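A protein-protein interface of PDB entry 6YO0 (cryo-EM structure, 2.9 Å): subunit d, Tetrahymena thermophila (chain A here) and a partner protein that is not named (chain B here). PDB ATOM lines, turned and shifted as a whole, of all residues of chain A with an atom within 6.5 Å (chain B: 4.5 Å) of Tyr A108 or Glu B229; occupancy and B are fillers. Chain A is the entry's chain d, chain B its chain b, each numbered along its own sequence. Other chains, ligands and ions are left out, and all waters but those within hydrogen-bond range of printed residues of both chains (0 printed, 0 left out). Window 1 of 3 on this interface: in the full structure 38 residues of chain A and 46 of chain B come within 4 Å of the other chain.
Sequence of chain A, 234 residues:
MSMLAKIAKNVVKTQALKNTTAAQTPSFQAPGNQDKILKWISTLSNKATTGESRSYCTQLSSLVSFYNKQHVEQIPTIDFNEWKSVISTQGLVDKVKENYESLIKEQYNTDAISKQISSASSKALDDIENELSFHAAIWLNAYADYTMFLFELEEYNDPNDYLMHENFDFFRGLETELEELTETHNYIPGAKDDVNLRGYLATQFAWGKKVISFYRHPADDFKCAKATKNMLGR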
ATOM      1  N   PHE A  66     -36.065 -16.496   1.600  1.00  0.00           N
ATOM      2  CA  PHE A  66     -35.465 -15.185   1.812  1.00  0.00           C
ATOM      3  C   PHE A  66     -34.342 -14.919   0.819  1.00  0.00           C
ATOM      4  O   PHE A  66     -34.250 -13.829   0.247  1.00  0.00           O
ATOM      5  CB  PHE A  66     -34.954 -15.080   3.245  1.00  0.00           C
ATOM      6  CG  PHE A  66     -34.033 -13.925   3.474  1.00  0.00           C
ATOM      7  CD1 PHE A  66     -34.531 -12.681   3.800  1.00  0.00           C
ATOM      8  CD2 PHE A  66     -32.665 -14.089   3.379  1.00  0.00           C
ATOM      9  CE1 PHE A  66     -33.682 -11.619   4.012  1.00  0.00           C
ATOM     10  CE2 PHE A  66     -31.811 -13.031   3.592  1.00  0.00           C
ATOM     11  CZ  PHE A  66     -32.320 -11.796   3.913  1.00  0.00           C
ATOM     12  N   LYS A  69     -35.758 -14.603  -2.925  1.00  0.00           N
ATOM     13  CA  LYS A  69     -36.803 -13.628  -3.209  1.00  0.00           C
ATOM     14  C   LYS A  69     -36.429 -12.805  -4.434  1.00  0.00           C
ATOM     15  O   LYS A  69     -35.377 -12.158  -4.462  1.00  0.00           O
ATOM     16  CB  LYS A  69     -37.028 -12.709  -2.008  1.00  0.00           C
ATOM     17  CG  LYS A  69     -35.817 -11.877  -1.606  1.00  0.00           C
ATOM     18  CD  LYS A  69     -36.111 -10.949  -0.432  1.00  0.00           C
ATOM     19  CE  LYS A  69     -36.590 -11.688   0.804  1.00  0.00           C
ATOM     20  NZ  LYS A  69     -36.877 -10.745   1.917  1.00  0.00           N
ATOM     21  N   HIS A  71     -36.837  -9.725  -7.123  1.00  0.00           N
ATOM     22  CA  HIS A  71     -37.195  -8.313  -7.090  1.00  0.00           C
ATOM     23  C   HIS A  71     -37.475  -7.833  -8.505  1.00  0.00           C
ATOM     24  O   HIS A  71     -36.612  -7.938  -9.382  1.00  0.00           O
ATOM     25  CB  HIS A  71     -36.080  -7.484  -6.462  1.00  0.00           C
ATOM     26  CG  HIS A  71     -36.265  -6.008  -6.624  1.00  0.00           C
ATOM     27  ND1 HIS A  71     -35.929  -5.339  -7.781  1.00  0.00           N
ATOM     28  CD2 HIS A  71     -36.751  -5.073  -5.776  1.00  0.00           C
ATOM     29  CE1 HIS A  71     -36.202  -4.055  -7.638  1.00  0.00           C
ATOM     30  NE2 HIS A  71     -36.702  -3.867  -6.431  1.00  0.00           N
ATOM     31  N   GLU A 106     -20.390   1.284  -8.036  1.00  0.00           N
ATOM     32  CA  GLU A 106     -20.154   0.243  -7.045  1.00  0.00           C
ATOM     33  C   GLU A 106     -21.092  -0.935  -7.268  1.00  0.00           C
ATOM     34  O   GLU A 106     -22.291  -0.762  -7.504  1.00  0.00           O
ATOM     35  CB  GLU A 106     -20.350   0.808  -5.639  1.00  0.00           C
ATOM     36  CG  GLU A 106     -19.413   1.951  -5.264  1.00  0.00           C
ATOM     37  CD  GLU A 106     -17.952   1.542  -5.193  1.00  0.00           C
ATOM     38  OE1 GLU A 106     -17.476   0.820  -6.091  1.00  0.00           O
ATOM     39  OE2 GLU A 106     -17.275   1.947  -4.225  1.00  0.00           O
ATOM     40  N   GLN A 107     -20.537  -2.143  -7.194  1.00  0.00           N
ATOM     41  CA  GLN A 107     -21.318  -3.355  -7.379  1.00  0.00           C
ATOM     42  C   GLN A 107     -20.727  -4.463  -6.522  1.00  0.00           C
ATOM     43  O   GLN A 107     -19.556  -4.420  -6.133  1.00  0.00           O
ATOM     44  CB  GLN A 107     -21.367  -3.778  -8.851  1.00  0.00           C
ATOM     45  CG  GLN A 107     -20.014  -4.073  -9.460  1.00  0.00           C
ATOM     46  CD  GLN A 107     -20.115  -4.499 -10.911  1.00  0.00           C
ATOM     47  OE1 GLN A 107     -21.210  -4.607 -11.463  1.00  0.00           O
ATOM     48  NE2 GLN A 107     -18.970  -4.741 -11.538  1.00  0.00           N
ATOM     49  N   TYR A 108     -21.561  -5.457  -6.229  1.00  0.00           N
ATOM     50  CA  TYR A 108     -21.122  -6.599  -5.441  1.00  0.00           C
ATOM     51  C   TYR A 108     -19.934  -7.274  -6.113  1.00  0.00           C
ATOM     52  O   TYR A 108     -19.761  -7.203  -7.332  1.00  0.00           O
ATOM     53  CB  TYR A 108     -22.255  -7.613  -5.273  1.00  0.00           C
ATOM     54  CG  TYR A 108     -23.483  -7.121  -4.528  1.00  0.00           C
ATOM     55  CD1 TYR A 108     -23.867  -7.704  -3.332  1.00  0.00           C
ATOM     56  CD2 TYR A 108     -24.280  -6.110  -5.042  1.00  0.00           C
ATOM     57  CE1 TYR A 108     -24.990  -7.274  -2.654  1.00  0.00           C
ATOM     58  CE2 TYR A 108     -25.403  -5.674  -4.372  1.00  0.00           C
ATOM     59  CZ  TYR A 108     -25.757  -6.263  -3.182  1.00  0.00           C
ATOM     60  OH  TYR A 108     -26.878  -5.829  -2.513  1.00  0.00           O
ATOM     61  N   ASN A 109     -19.092  -7.912  -5.306  1.00  0.00           N
ATOM     62  CA  ASN A 109     -17.980  -8.716  -5.807  1.00  0.00           C
ATOM     63  C   ASN A 109     -18.337 -10.189  -5.609  1.00  0.00           C
ATOM     64  O   ASN A 109     -17.924 -10.825  -4.640  1.00  0.00           O
ATOM     65  CB  ASN A 109     -16.682  -8.347  -5.092  1.00  0.00           C
ATOM     66  CG  ASN A 109     -16.825  -8.353  -3.584  1.00  0.00           C
ATOM     67  OD1 ASN A 109     -17.871  -8.720  -3.051  1.00  0.00           O
ATOM     68  ND2 ASN A 109     -15.769  -7.952  -2.888  1.00  0.00           N
ATOM     69  N   THR A 110     -19.094 -10.740  -6.561  1.00  0.00           N
ATOM     70  CA  THR A 110     -19.550 -12.119  -6.425  1.00  0.00           C
ATOM     71  C   THR A 110     -18.387 -13.098  -6.376  1.00  0.00           C
ATOM     72  O   THR A 110     -18.492 -14.156  -5.746  1.00  0.00           O
ATOM     73  CB  THR A 110     -20.474 -12.498  -7.583  1.00  0.00           C
ATOM     74  OG1 THR A 110     -19.815 -12.242  -8.829  1.00  0.00           O
ATOM     75  CG2 THR A 110     -21.760 -11.701  -7.524  1.00  0.00           C
ATOM     76  N   ASP A 111     -17.273 -12.765  -7.027  1.00  0.00           N
ATOM     77  CA  ASP A 111     -16.140 -13.682  -7.059  1.00  0.00           C
ATOM     78  C   ASP A 111     -15.610 -13.954  -5.657  1.00  0.00           C
ATOM     79  O   ASP A 111     -15.411 -15.111  -5.272  1.00  0.00           O
ATOM     80  CB  ASP A 111     -15.037 -13.111  -7.950  1.00  0.00           C
ATOM     81  CG  ASP A 111     -13.963 -14.130  -8.279  1.00  0.00           C
ATOM     82  OD1 ASP A 111     -13.761 -15.069  -7.481  1.00  0.00           O
ATOM     83  OD2 ASP A 111     -13.322 -13.994  -9.342  1.00  0.00           O
ATOM     84  N   ILE A 113     -17.057 -13.634  -2.684  1.00  0.00           N
ATOM     85  CA  ILE A 113     -18.020 -14.380  -1.881  1.00  0.00           C
ATOM     86  C   ILE A 113     -18.104 -15.832  -2.334  1.00  0.00           C
ATOM     87  O   ILE A 113     -18.141 -16.754  -1.511  1.00  0.00           O
ATOM     88  CB  ILE A 113     -19.401 -13.699  -1.931  1.00  0.00           C
ATOM     89  CG1 ILE A 113     -19.403 -12.403  -1.110  1.00  0.00           C
ATOM     90  CG2 ILE A 113     -20.479 -14.651  -1.441  1.00  0.00           C
ATOM     91  CD1 ILE A 113     -18.607 -11.269  -1.706  1.00  0.00           C
ATOM     92  N   LYS B  35     -22.739 -10.777 -13.286  1.00  0.00           N
ATOM     93  CA  LYS B  35     -22.387 -11.233 -11.949  1.00  0.00           C
ATOM     94  C   LYS B  35     -22.903 -12.646 -11.716  1.00  0.00           C
ATOM     95  O   LYS B  35     -22.244 -13.462 -11.062  1.00  0.00           O
ATOM     96  CB  LYS B  35     -22.969 -10.276 -10.908  1.00  0.00           C
ATOM     97  CG  LYS B  35     -22.312  -8.890 -10.796  1.00  0.00           C
ATOM     98  CD  LYS B  35     -20.794  -8.870 -10.932  1.00  0.00           C
ATOM     99  CE  LYS B  35     -20.132  -9.179  -9.609  1.00  0.00           C
ATOM    100  NZ  LYS B  35     -18.669  -8.912  -9.625  1.00  0.00           N
ATOM    101  N   PHE B 225     -29.669 -14.475  -4.642  1.00  0.00           N
ATOM    102  CA  PHE B 225     -29.863 -13.505  -3.572  1.00  0.00           C
ATOM    103  C   PHE B 225     -29.092 -12.222  -3.847  1.00  0.00           C
ATOM    104  O   PHE B 225     -29.641 -11.119  -3.746  1.00  0.00           O
ATOM    105  CB  PHE B 225     -29.432 -14.127  -2.246  1.00  0.00           C
ATOM    106  CG  PHE B 225     -29.275 -13.144  -1.130  1.00  0.00           C
ATOM    107  CD1 PHE B 225     -30.381 -12.625  -0.487  1.00  0.00           C
ATOM    108  CD2 PHE B 225     -28.019 -12.767  -0.700  1.00  0.00           C
ATOM    109  CE1 PHE B 225     -30.238 -11.729   0.550  1.00  0.00           C
ATOM    110  CE2 PHE B 225     -27.870 -11.874   0.338  1.00  0.00           C
ATOM    111  CZ  PHE B 225     -28.982 -11.353   0.963  1.00  0.00           C
ATOM    112  N   LEU B 226     -27.815 -12.345  -4.210  1.00  0.00           N
ATOM    113  CA  LEU B 226     -27.019 -11.159  -4.502  1.00  0.00           C
ATOM    114  C   LEU B 226     -27.565 -10.413  -5.709  1.00  0.00           C
ATOM    115  O   LEU B 226     -27.628  -9.179  -5.711  1.00  0.00           O
ATOM    116  CB  LEU B 226     -25.562 -11.546  -4.736  1.00  0.00           C
ATOM    117  CG  LEU B 226     -24.787 -12.036  -3.515  1.00  0.00           C
ATOM    118  CD1 LEU B 226     -23.335 -12.245  -3.884  1.00  0.00           C
ATOM    119  CD2 LEU B 226     -24.913 -11.069  -2.355  1.00  0.00           C
ATOM    120  N   ALA B 227     -27.967 -11.147  -6.746  1.00  0.00           N
ATOM    121  CA  ALA B 227     -28.495 -10.501  -7.941  1.00  0.00           C
ATOM    122  C   ALA B 227     -29.761  -9.720  -7.621  1.00  0.00           C
ATOM    123  O   ALA B 227     -29.863  -8.525  -7.923  1.00  0.00           O
ATOM    124  CB  ALA B 227     -28.767 -11.550  -9.016  1.00  0.00           C
ATOM    125  N   ASN B 228     -30.742 -10.381  -7.005  1.00  0.00           N
ATOM    126  CA  ASN B 228     -31.984  -9.697  -6.673  1.00  0.00           C
ATOM    127  C   ASN B 228     -31.746  -8.587  -5.662  1.00  0.00           C
ATOM    128  O   ASN B 228     -32.418  -7.551  -5.705  1.00  0.00           O
ATOM    129  CB  ASN B 228     -33.002 -10.701  -6.137  1.00  0.00           C
ATOM    130  CG  ASN B 228     -33.473 -11.670  -7.197  1.00  0.00           C
ATOM    131  OD1 ASN B 228     -33.289 -12.879  -7.076  1.00  0.00           O
ATOM    132  ND2 ASN B 228     -34.081 -11.142  -8.250  1.00  0.00           N
ATOM    133  N   GLU B 229     -30.793  -8.784  -4.748  1.00  0.00           N
ATOM    134  CA  GLU B 229     -30.487  -7.753  -3.765  1.00  0.00           C
ATOM    135  C   GLU B 229     -29.820  -6.555  -4.424  1.00  0.00           C
ATOM    136  O   GLU B 229     -30.078  -5.406  -4.050  1.00  0.00           O
ATOM    137  CB  GLU B 229     -29.595  -8.330  -2.670  1.00  0.00           C
ATOM    138  CG  GLU B 229     -29.515  -7.476  -1.426  1.00  0.00           C
ATOM    139  CD  GLU B 229     -30.802  -7.477  -0.630  1.00  0.00           C
ATOM    140  OE1 GLU B 229     -31.827  -7.974  -1.142  1.00  0.00           O
ATOM    141  OE2 GLU B 229     -30.790  -6.980   0.516  1.00  0.00           O
ATOM    142  N   TYR B 230     -28.956  -6.809  -5.408  1.00  0.00           N
ATOM    143  CA  TYR B 230     -28.349  -5.720  -6.162  1.00  0.00           C
ATOM    144  C   TYR B 230     -29.410  -4.905  -6.886  1.00  0.00           C
ATOM    145  O   TYR B 230     -29.357  -3.670  -6.899  1.00  0.00           O
ATOM    146  CB  TYR B 230     -27.336  -6.293  -7.151  1.00  0.00           C
ATOM    147  CG  TYR B 230     -26.702  -5.285  -8.080  1.00  0.00           C
ATOM    148  CD1 TYR B 230     -25.630  -4.509  -7.671  1.00  0.00           C
ATOM    149  CD2 TYR B 230     -27.163  -5.133  -9.378  1.00  0.00           C
ATOM    150  CE1 TYR B 230     -25.047  -3.595  -8.524  1.00  0.00           C
ATOM    151  CE2 TYR B 230     -26.584  -4.226 -10.238  1.00  0.00           C
ATOM    152  CZ  TYR B 230     -25.525  -3.462  -9.807  1.00  0.00           C
ATOM    153  OH  TYR B 230     -24.948  -2.555 -10.661  1.00  0.00           O
ATOM    154  N   LEU B 231     -30.385  -5.582  -7.492  1.00  0.00           N
ATOM    155  CA  LEU B 231     -31.482  -4.875  -8.142  1.00  0.00           C
ATOM    156  C   LEU B 231     -32.259  -4.027  -7.144  1.00  0.00           C
ATOM    157  O   LEU B 231     -32.619  -2.882  -7.438  1.00  0.00           O
ATOM    158  CB  LEU B 231     -32.411  -5.874  -8.828  1.00  0.00           C
ATOM    159  CG  LEU B 231     -31.916  -6.494 -10.137  1.00  0.00           C
ATOM    160  CD1 LEU B 231     -33.034  -7.276 -10.803  1.00  0.00           C
ATOM    161  CD2 LEU B 231     -31.364  -5.449 -11.082  1.00  0.00           C
ATOM    162  N   ARG B 232     -32.527  -4.571  -5.954  1.00  0.00           N
ATOM    163  CA  ARG B 232     -33.281  -3.819  -4.957  1.00  0.00           C
ATOM    164  C   ARG B 232     -32.517  -2.583  -4.514  1.00  0.00           C
ATOM    165  O   ARG B 232     -33.105  -1.514  -4.313  1.00  0.00           O
ATOM    166  CB  ARG B 232     -33.578  -4.699  -3.745  1.00  0.00           C
ATOM    167  CG  ARG B 232     -34.485  -4.035  -2.727  1.00  0.00           C
ATOM    168  CD  ARG B 232     -34.910  -4.999  -1.633  1.00  0.00           C
ATOM    169  NE  ARG B 232     -33.788  -5.383  -0.779  1.00  0.00           N
ATOM    170  CZ  ARG B 232     -33.480  -4.783   0.369  1.00  0.00           C
ATOM    171  NH1 ARG B 232     -34.200  -3.763   0.814  1.00  0.00           N
ATOM    172  NH2 ARG B 232     -32.443  -5.203   1.079  1.00  0.00           N
ATOM    173  N   LEU B 233     -31.200  -2.708  -4.360  1.00  0.00           N
ATOM    174  CA  LEU B 233     -30.392  -1.563  -3.968  1.00  0.00           C
ATOM    175  C   LEU B 233     -30.373  -0.503  -5.059  1.00  0.00           C
ATOM    176  O   LEU B 233     -30.437   0.698  -4.768  1.00  0.00           O
ATOM    177  CB  LEU B 233     -28.974  -2.024  -3.646  1.00  0.00           C
ATOM    178  CG  LEU B 233     -27.947  -0.933  -3.344  1.00  0.00           C
ATOM    179  CD1 LEU B 233     -26.907  -1.468  -2.384  1.00  0.00           C
ATOM    180  CD2 LEU B 233     -27.286  -0.424  -4.614  1.00  0.00           C
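The side-chain carboxylate (OE2) of Glu B229 lies within salt-bridge range of the guanidinium group (NH2) of Arg B232, 2.5 Å away.
Phe A66 touches Phe B225.
Leu B231 touches His A71.
NE2 of His A71 touches CA of Arg B232 (3.7 Å).
CB of Gln A107 touches CE1 of Tyr B230, at 3.7 Å.
Leu B226 touches Tyr A108.
Tyr A108 touches Glu B229 (OH to CG, 3.3 Å).
CD1 of Tyr B230 touches CD2 of Tyr A108, at 3.4 Å.
CA of Asn A109 touches NZ of Lys B35 (3.9 Å).
OG1 of Thr A110 touches CE of Lys B35, 3.2 Å away.
Of the 10 printed residues of chain A, 7 touch a printed residue of chain B.
Printed residues of chain B that touch a printed residue of chain A: Lys B35, Phe B225, Leu B226, Asn B228, Glu B229, Tyr B230, Leu B231 and Arg B232.
Hydrophobic or aromatic side chains of chain B that line the printed part of chain A: Phe B225, Leu B226, Tyr B230 and Leu B231.
Among the printed residues, no Asp or Glu carboxylate lies within 4 Å of a Lys or Arg side-chain nitrogen of the other chain.
N of His A71 sits close to ND2 of Asn B228, 3.3 Å away.
NZ of Lys B35 lies close to O of Tyr A108 (3.1 Å).
The side-chain amide oxygen (OD1) of Asn B228 lies close to the backbone carbonyl oxygen (O) of Lys A69 (3.4 Å).
Glu A106 touches none of the printed residues of chain B.
Of the printed residues of chain B, Gln A107 touches Tyr B230 (3.7 Å).
Of the printed residues of chain B, Tyr A108 touches Lys B35 (3.0 Å), Leu B226 (3.7 Å), Glu B229 (3.3 Å) and Tyr B230 (3.4 Å).
Of the printed residues of chain A, Leu B226 touches Tyr A108.
Glu B229 touches just one residue of chain A: Tyr A108.
Of the printed residues of chain A, Tyr B230 touches Gln A107 and Tyr A108.
Of the printed residues of chain A, Leu B231 touches His A71.
Of the printed residues of chain A, Arg B232 touches His A71.
Leu B233 touches none of the printed residues of chain A.
The nearest residue of chain B that does not touch Tyr A108 is Leu B233 (4.4 Å).
The nearest printed residue of chain A that does not touch Asn B228 is Tyr A108 (6.4 Å).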
